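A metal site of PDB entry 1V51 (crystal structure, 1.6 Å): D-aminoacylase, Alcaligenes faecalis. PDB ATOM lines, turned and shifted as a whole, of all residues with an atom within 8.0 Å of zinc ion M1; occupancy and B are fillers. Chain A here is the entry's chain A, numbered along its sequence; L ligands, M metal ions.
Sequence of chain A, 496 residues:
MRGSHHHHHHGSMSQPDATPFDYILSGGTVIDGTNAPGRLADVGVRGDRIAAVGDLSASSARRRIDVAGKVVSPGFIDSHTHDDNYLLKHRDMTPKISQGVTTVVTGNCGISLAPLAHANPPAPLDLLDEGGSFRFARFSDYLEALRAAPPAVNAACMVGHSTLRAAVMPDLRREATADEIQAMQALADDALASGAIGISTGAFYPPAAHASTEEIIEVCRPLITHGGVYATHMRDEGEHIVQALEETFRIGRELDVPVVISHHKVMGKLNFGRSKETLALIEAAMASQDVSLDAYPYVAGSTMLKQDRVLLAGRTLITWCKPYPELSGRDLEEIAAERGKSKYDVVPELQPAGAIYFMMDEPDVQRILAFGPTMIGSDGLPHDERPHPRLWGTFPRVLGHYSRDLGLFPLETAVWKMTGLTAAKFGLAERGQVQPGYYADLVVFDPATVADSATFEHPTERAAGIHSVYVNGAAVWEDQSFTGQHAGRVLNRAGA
The backbone carbonyl oxygen (O) of Thr 201 sits at hydrogen-bond distance from the backbone NH (N) of His 233 (2.9 Å). ND1 of His 263 lies within hydrogen-bond range of OE2 of Glu 237 (3.1 Å). The side-chain amino group (NZ) of Lys 265 is in hydrogen-bond range of the backbone carbonyl oxygen (O) of His 263, 3.1 Å away.
Zinc ion M1 is bound by a ring nitrogen (ND1) of His 233 (2.0 Å), a ring nitrogen (NE2) of His 263 (2.0 Å), an oxygen (O1) of the ligand (2.1 Å), the side-chain sulfur of Cys 109 (2.3 Å) and an oxygen (O2) of the ligand (2.5 Å). Zinc ion M1 has five donor atoms within binding distance.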
ATOM      1  N   HIS A  80     -16.244 -28.225  12.451  1.00  0.00           N
ATOM      2  CA  HIS A  80     -15.184 -27.544  13.178  1.00  0.00           C
ATOM      3  C   HIS A  80     -15.234 -27.851  14.662  1.00  0.00           C
ATOM      4  O   HIS A  80     -16.044 -27.268  15.393  1.00  0.00           O
ATOM      5  CB  HIS A  80     -15.312 -26.024  12.987  1.00  0.00           C
ATOM      6  CG  HIS A  80     -14.168 -25.258  13.579  1.00  0.00           C
ATOM      7  ND1 HIS A  80     -13.068 -24.874  12.843  1.00  0.00           N
ATOM      8  CD2 HIS A  80     -13.940 -24.829  14.846  1.00  0.00           C
ATOM      9  CE1 HIS A  80     -12.206 -24.254  13.637  1.00  0.00           C
ATOM     10  NE2 HIS A  80     -12.708 -24.218  14.856  1.00  0.00           N
ATOM     11  N   HIS A  82     -12.926 -29.093  18.440  1.00  0.00           N
ATOM     12  CA  HIS A  82     -11.691 -29.190  19.192  1.00  0.00           C
ATOM     13  C   HIS A  82     -11.892 -30.385  20.129  1.00  0.00           C
ATOM     14  O   HIS A  82     -11.621 -30.323  21.337  1.00  0.00           O
ATOM     15  CB  HIS A  82     -11.409 -27.895  19.945  1.00  0.00           C
ATOM     16  CG  HIS A  82     -11.079 -26.758  19.025  1.00  0.00           C
ATOM     17  ND1 HIS A  82      -9.925 -26.718  18.281  1.00  0.00           N
ATOM     18  CD2 HIS A  82     -11.813 -25.684  18.651  1.00  0.00           C
ATOM     19  CE1 HIS A  82      -9.950 -25.664  17.482  1.00  0.00           C
ATOM     20  NE2 HIS A  82     -11.101 -25.021  17.691  1.00  0.00           N
ATOM     21  N   ASN A 108      -8.283 -28.512  14.546  1.00  0.00           N
ATOM     22  CA  ASN A 108      -8.520 -27.243  13.880  1.00  0.00           C
ATOM     23  C   ASN A 108      -7.688 -26.068  14.401  1.00  0.00           C
ATOM     24  O   ASN A 108      -7.172 -26.096  15.515  1.00  0.00           O
ATOM     25  CB  ASN A 108     -10.009 -26.933  14.011  1.00  0.00           C
ATOM     26  CG  ASN A 108     -10.838 -27.785  13.099  1.00  0.00           C
ATOM     27  OD1 ASN A 108     -11.504 -28.748  13.525  1.00  0.00           O
ATOM     28  ND2 ASN A 108     -10.785 -27.476  11.823  1.00  0.00           N
ATOM     29  N   CYS A 109      -7.565 -25.028  13.566  1.00  0.00           N
ATOM     30  CA  CYS A 109      -6.864 -23.797  13.898  1.00  0.00           C
ATOM     31  C   CYS A 109      -5.407 -23.998  14.256  1.00  0.00           C
ATOM     32  O   CYS A 109      -4.853 -23.216  15.046  1.00  0.00           O
ATOM     33  CB  CYS A 109      -7.571 -23.099  15.065  1.00  0.00           C
ATOM     34  SG  CYS A 109      -9.356 -22.938  14.747  1.00  0.00           S
ATOM     35  N   GLY A 110      -4.795 -25.018  13.649  1.00  0.00           N
ATOM     36  CA  GLY A 110      -3.402 -25.339  13.905  1.00  0.00           C
ATOM     37  C   GLY A 110      -3.194 -26.085  15.206  1.00  0.00           C
ATOM     38  O   GLY A 110      -2.058 -26.410  15.552  1.00  0.00           O
ATOM     39  N   ILE A 111      -4.295 -26.384  15.895  1.00  0.00           N
ATOM     40  CA  ILE A 111      -4.278 -27.071  17.197  1.00  0.00           C
ATOM     41  C   ILE A 111      -4.675 -28.545  17.153  1.00  0.00           C
ATOM     42  O   ILE A 111      -5.857 -28.855  17.006  1.00  0.00           O
ATOM     43  CB  ILE A 111      -5.264 -26.403  18.189  1.00  0.00           C
ATOM     44  CG1 ILE A 111      -5.026 -24.886  18.264  1.00  0.00           C
ATOM     45  CG2 ILE A 111      -5.103 -27.031  19.575  1.00  0.00           C
ATOM     46  CD1 ILE A 111      -6.198 -24.162  18.952  1.00  0.00           C
ATOM     47  N   PRO A 124      -2.829 -21.516  22.358  1.00  0.00           N
ATOM     48  CA  PRO A 124      -4.091 -22.147  22.748  1.00  0.00           C
ATOM     49  C   PRO A 124      -4.125 -23.679  22.734  1.00  0.00           C
ATOM     50  O   PRO A 124      -5.202 -24.274  22.780  1.00  0.00           O
ATOM     51  CB  PRO A 124      -5.071 -21.552  21.743  1.00  0.00           C
ATOM     52  CG  PRO A 124      -4.237 -21.542  20.478  1.00  0.00           C
ATOM     53  CD  PRO A 124      -2.913 -20.994  20.984  1.00  0.00           C
ATOM     54  N   LEU A 127      -6.214 -25.674  25.191  1.00  0.00           N
ATOM     55  CA  LEU A 127      -7.663 -25.853  25.075  1.00  0.00           C
ATOM     56  C   LEU A 127      -8.040 -27.334  24.967  1.00  0.00           C
ATOM     57  O   LEU A 127      -9.204 -27.695  25.155  1.00  0.00           O
ATOM     58  CB  LEU A 127      -8.207 -25.097  23.872  1.00  0.00           C
ATOM     59  CG  LEU A 127      -8.276 -23.574  24.002  1.00  0.00           C
ATOM     60  CD1 LEU A 127      -8.761 -22.976  22.702  1.00  0.00           C
ATOM     61  CD2 LEU A 127      -9.211 -23.191  25.159  1.00  0.00           C
ATOM     62  N   THR A 201      -4.046 -24.538  10.167  1.00  0.00           N
ATOM     63  CA  THR A 201      -3.162 -23.506  10.707  1.00  0.00           C
ATOM     64  C   THR A 201      -3.986 -22.477  11.479  1.00  0.00           C
ATOM     65  O   THR A 201      -5.218 -22.401  11.327  1.00  0.00           O
ATOM     66  CB  THR A 201      -2.418 -22.736   9.613  1.00  0.00           C
ATOM     67  OG1 THR A 201      -3.387 -22.052   8.809  1.00  0.00           O
ATOM     68  CG2 THR A 201      -1.587 -23.680   8.748  1.00  0.00           C
ATOM     69  N   GLY A 202      -3.290 -21.709  12.296  1.00  0.00           N
ATOM     70  CA  GLY A 202      -3.910 -20.660  13.088  1.00  0.00           C
ATOM     71  C   GLY A 202      -2.842 -19.627  13.412  1.00  0.00           C
ATOM     72  O   GLY A 202      -2.453 -19.476  14.577  1.00  0.00           O
ATOM     73  N   PHE A 204      -3.025 -16.628  13.727  1.00  0.00           N
ATOM     74  CA  PHE A 204      -3.538 -15.567  14.592  1.00  0.00           C
ATOM     75  C   PHE A 204      -2.968 -15.772  16.007  1.00  0.00           C
ATOM     76  O   PHE A 204      -2.723 -14.801  16.759  1.00  0.00           O
ATOM     77  CB  PHE A 204      -5.073 -15.682  14.661  1.00  0.00           C
ATOM     78  CG  PHE A 204      -5.699 -14.892  15.785  1.00  0.00           C
ATOM     79  CD1 PHE A 204      -5.861 -13.516  15.665  1.00  0.00           C
ATOM     80  CD2 PHE A 204      -6.146 -15.519  16.937  1.00  0.00           C
ATOM     81  CE1 PHE A 204      -6.467 -12.782  16.680  1.00  0.00           C
ATOM     82  CE2 PHE A 204      -6.755 -14.792  17.958  1.00  0.00           C
ATOM     83  CZ  PHE A 204      -6.917 -13.417  17.821  1.00  0.00           C
ATOM     84  N   TYR A 205      -2.720 -17.029  16.373  1.00  0.00           N
ATOM     85  CA  TYR A 205      -2.224 -17.362  17.722  1.00  0.00           C
ATOM     86  C   TYR A 205      -0.708 -17.260  17.930  1.00  0.00           C
ATOM     87  O   TYR A 205       0.072 -17.408  16.998  1.00  0.00           O
ATOM     88  CB  TYR A 205      -2.713 -18.756  18.116  1.00  0.00           C
ATOM     89  CG  TYR A 205      -4.231 -18.803  18.294  1.00  0.00           C
ATOM     90  CD1 TYR A 205      -4.837 -18.154  19.356  1.00  0.00           C
ATOM     91  CD2 TYR A 205      -5.049 -19.477  17.373  1.00  0.00           C
ATOM     92  CE1 TYR A 205      -6.229 -18.161  19.520  1.00  0.00           C
ATOM     93  CE2 TYR A 205      -6.441 -19.484  17.519  1.00  0.00           C
ATOM     94  CZ  TYR A 205      -7.022 -18.832  18.598  1.00  0.00           C
ATOM     95  OH  TYR A 205      -8.386 -18.865  18.779  1.00  0.00           O
ATOM     96  N   THR A 232      -8.035 -23.365   7.868  1.00  0.00           N
ATOM     97  CA  THR A 232      -7.384 -22.249   8.537  1.00  0.00           C
ATOM     98  C   THR A 232      -8.210 -21.311   9.397  1.00  0.00           C
ATOM     99  O   THR A 232      -9.329 -20.949   9.055  1.00  0.00           O
ATOM    100  CB  THR A 232      -6.653 -21.372   7.482  1.00  0.00           C
ATOM    101  OG1 THR A 232      -5.967 -20.281   8.139  1.00  0.00           O
ATOM    102  CG2 THR A 232      -7.647 -20.757   6.494  1.00  0.00           C
ATOM    103  N   HIS A 233      -7.614 -20.940  10.527  1.00  0.00           N
ATOM    104  CA  HIS A 233      -8.142 -19.895  11.381  1.00  0.00           C
ATOM    105  C   HIS A 233      -7.289 -18.774  10.782  1.00  0.00           C
ATOM    106  O   HIS A 233      -6.080 -18.731  11.002  1.00  0.00           O
ATOM    107  CB  HIS A 233      -7.761 -20.125  12.845  1.00  0.00           C
ATOM    108  CG  HIS A 233      -8.150 -18.994  13.748  1.00  0.00           C
ATOM    109  ND1 HIS A 233      -8.759 -19.210  14.966  1.00  0.00           N
ATOM    110  CD2 HIS A 233      -8.009 -17.653  13.619  1.00  0.00           C
ATOM    111  CE1 HIS A 233      -8.976 -18.037  15.560  1.00  0.00           C
ATOM    112  NE2 HIS A 233      -8.519 -17.085  14.767  1.00  0.00           N
ATOM    113  N   MET A 234      -7.901 -17.884  10.011  1.00  0.00           N
ATOM    114  CA  MET A 234      -7.128 -16.835   9.328  1.00  0.00           C
ATOM    115  C   MET A 234      -6.297 -15.961  10.235  1.00  0.00           C
ATOM    116  O   MET A 234      -6.614 -15.773  11.409  1.00  0.00           O
ATOM    117  CB  MET A 234      -8.049 -16.042   8.401  1.00  0.00           C
ATOM    118  CG  MET A 234      -8.653 -16.945   7.312  1.00  0.00           C
ATOM    119  SD  MET A 234      -9.559 -16.012   6.077  1.00  0.00           S
ATOM    120  CE  MET A 234     -10.848 -15.259   7.107  1.00  0.00           C
ATOM    121  N   GLU A 237      -9.164 -11.622  11.603  1.00  0.00           N
ATOM    122  CA  GLU A 237     -10.574 -11.694  11.237  1.00  0.00           C
ATOM    123  C   GLU A 237     -11.284 -10.354  11.494  1.00  0.00           C
ATOM    124  O   GLU A 237     -12.505 -10.309  11.649  1.00  0.00           O
ATOM    125  CB  GLU A 237     -11.261 -12.811  12.017  1.00  0.00           C
ATOM    126  CG  GLU A 237     -10.710 -14.210  11.716  1.00  0.00           C
ATOM    127  CD  GLU A 237     -11.527 -15.306  12.400  1.00  0.00           C
ATOM    128  OE1 GLU A 237     -11.556 -15.322  13.648  1.00  0.00           O
ATOM    129  OE2 GLU A 237     -12.148 -16.150  11.698  1.00  0.00           O
ATOM    130  N   SER A 262     -12.119 -21.457   8.477  1.00  0.00           N
ATOM    131  CA  SER A 262     -12.816 -21.767   9.732  1.00  0.00           C
ATOM    132  C   SER A 262     -13.557 -20.603  10.362  1.00  0.00           C
ATOM    133  O   SER A 262     -13.095 -19.464  10.311  1.00  0.00           O
ATOM    134  CB  SER A 262     -11.821 -22.260  10.787  1.00  0.00           C
ATOM    135  OG  SER A 262     -11.113 -23.397  10.342  1.00  0.00           O
ATOM    136  N   HIS A 263     -14.678 -20.947  11.017  1.00  0.00           N
ATOM    137  CA  HIS A 263     -15.507 -19.997  11.755  1.00  0.00           C
ATOM    138  C   HIS A 263     -15.498 -18.596  11.170  1.00  0.00           C
ATOM    139  O   HIS A 263     -15.043 -17.655  11.816  1.00  0.00           O
ATOM    140  CB  HIS A 263     -15.113 -19.975  13.268  1.00  0.00           C
ATOM    141  CG  HIS A 263     -13.638 -19.877  13.552  1.00  0.00           C
ATOM    142  ND1 HIS A 263     -12.834 -18.851  13.095  1.00  0.00           N
ATOM    143  CD2 HIS A 263     -12.832 -20.648  14.325  1.00  0.00           C
ATOM    144  CE1 HIS A 263     -11.602 -19.001  13.559  1.00  0.00           C
ATOM    145  NE2 HIS A 263     -11.575 -20.084  14.324  1.00  0.00           N
ATOM    146  N   LYS A 265     -16.263 -14.959  10.197  1.00  0.00           N
ATOM    147  CA  LYS A 265     -16.885 -13.860  10.931  1.00  0.00           C
ATOM    148  C   LYS A 265     -16.151 -12.563  10.620  1.00  0.00           C
ATOM    149  O   LYS A 265     -15.091 -12.558   9.982  1.00  0.00           O
ATOM    150  CB  LYS A 265     -16.711 -14.103  12.433  1.00  0.00           C
ATOM    151  CG  LYS A 265     -15.202 -14.035  12.833  1.00  0.00           C
ATOM    152  CD  LYS A 265     -14.970 -14.079  14.343  1.00  0.00           C
ATOM    153  CE  LYS A 265     -15.164 -15.442  14.906  1.00  0.00           C
ATOM    154  NZ  LYS A 265     -14.095 -16.415  14.443  1.00  0.00           N
ATOM    155  N   TYR A 296     -20.323 -20.915  13.139  1.00  0.00           N
ATOM    156  CA  TYR A 296     -21.187 -21.350  14.230  1.00  0.00           C
ATOM    157  C   TYR A 296     -22.262 -20.246  14.329  1.00  0.00           C
ATOM    158  O   TYR A 296     -22.017 -19.067  14.038  1.00  0.00           O
ATOM    159  CB  TYR A 296     -20.397 -21.548  15.539  1.00  0.00           C
ATOM    160  CG  TYR A 296     -19.511 -20.404  15.933  1.00  0.00           C
ATOM    161  CD1 TYR A 296     -20.030 -19.282  16.583  1.00  0.00           C
ATOM    162  CD2 TYR A 296     -18.141 -20.444  15.649  1.00  0.00           C
ATOM    163  CE1 TYR A 296     -19.193 -18.215  16.956  1.00  0.00           C
ATOM    164  CE2 TYR A 296     -17.295 -19.390  16.010  1.00  0.00           C
ATOM    165  CZ  TYR A 296     -17.837 -18.284  16.661  1.00  0.00           C
ATOM    166  OH  TYR A 296     -16.998 -17.246  17.017  1.00  0.00           O
ATOM    167  N   SER A 302     -15.073 -17.765  21.328  1.00  0.00           N
ATOM    168  CA  SER A 302     -14.477 -18.303  22.546  1.00  0.00           C
ATOM    169  C   SER A 302     -13.149 -18.966  22.207  1.00  0.00           C
ATOM    170  O   SER A 302     -13.027 -19.655  21.198  1.00  0.00           O
ATOM    171  CB  SER A 302     -15.422 -19.319  23.207  1.00  0.00           C
ATOM    172  OG  SER A 302     -14.903 -19.772  24.453  1.00  0.00           O
ATOM    173  N   THR A 303     -12.134 -18.728  23.050  1.00  0.00           N
ATOM    174  CA  THR A 303     -10.805 -19.303  22.855  1.00  0.00           C
ATOM    175  C   THR A 303      -9.964 -18.908  24.068  1.00  0.00           C
ATOM    176  O   THR A 303     -10.523 -18.567  25.093  1.00  0.00           O
ATOM    177  CB  THR A 303     -10.144 -18.799  21.534  1.00  0.00           C
ATOM    178  OG1 THR A 303      -8.884 -19.459  21.381  1.00  0.00           O
ATOM    179  CG2 THR A 303      -9.944 -17.280  21.540  1.00  0.00           C
ATOM    180  N   ASP A 379     -17.502 -25.425  16.942  1.00  0.00           N
ATOM    181  CA  ASP A 379     -16.348 -24.792  17.593  1.00  0.00           C
ATOM    182  C   ASP A 379     -16.473 -24.992  19.116  1.00  0.00           C
ATOM    183  O   ASP A 379     -16.009 -24.170  19.907  1.00  0.00           O
ATOM    184  CB  ASP A 379     -16.241 -23.300  17.260  1.00  0.00           C
ATOM    185  CG  ASP A 379     -14.804 -22.803  17.309  1.00  0.00           C
ATOM    186  OD1 ASP A 379     -13.920 -23.600  17.671  1.00  0.00           O
ATOM    187  OD2 ASP A 379     -14.567 -21.626  16.978  1.00  0.00           O
ATOM    188  N   LEU A 381     -15.667 -26.034  22.814  1.00  0.00           N
ATOM    189  CA  LEU A 381     -14.397 -26.192  23.579  1.00  0.00           C
ATOM    190  C   LEU A 381     -14.889 -27.022  24.757  1.00  0.00           C
ATOM    191  O   LEU A 381     -15.253 -26.491  25.823  1.00  0.00           O
ATOM    192  CB  LEU A 381     -13.857 -24.819  23.998  1.00  0.00           C
ATOM    193  CG  LEU A 381     -13.639 -23.824  22.838  1.00  0.00           C
ATOM    194  CD1 LEU A 381     -13.023 -22.542  23.338  1.00  0.00           C
ATOM    195  CD2 LEU A 381     -12.707 -24.455  21.812  1.00  0.00           C
ATOM    196  N   ARG A 390     -22.413 -22.994  22.388  1.00  0.00           N
ATOM    197  CA  ARG A 390     -22.329 -23.591  21.049  1.00  0.00           C
ATOM    198  C   ARG A 390     -21.921 -25.056  21.161  1.00  0.00           C
ATOM    199  O   ARG A 390     -22.210 -25.884  20.275  1.00  0.00           O
ATOM    200  CB  ARG A 390     -21.323 -22.813  20.176  1.00  0.00           C
ATOM    201  CG  ARG A 390     -19.880 -22.857  20.671  1.00  0.00           C
ATOM    202  CD  ARG A 390     -19.062 -21.762  19.987  1.00  0.00           C
ATOM    203  NE  ARG A 390     -17.630 -21.895  20.246  1.00  0.00           N
ATOM    204  CZ  ARG A 390     -16.728 -20.979  19.892  1.00  0.00           C
ATOM    205  NH1 ARG A 390     -17.113 -19.866  19.288  1.00  0.00           N
ATOM    206  NH2 ARG A 390     -15.438 -21.220  20.091  1.00  0.00           N
HETATM  207  C1  LIG L   1     -10.662 -21.367  17.781  1.00  0.00           C
HETATM  208  O1  LIG L   1      -9.784 -20.553  17.423  1.00  0.00           O
HETATM  209  O2  LIG L   1     -11.535 -21.789  17.008  1.00  0.00           O
HETATM  210  C2  LIG L   1     -10.745 -21.763  19.237  1.00  0.00           C
HETATM  211 ZN    ZN M   1      -9.957 -20.815  15.345  1.00  0.00          ZN
HETATM  212 ZN    ZN M   2     -12.203 -23.599  16.717  1.00  0.00          ZN
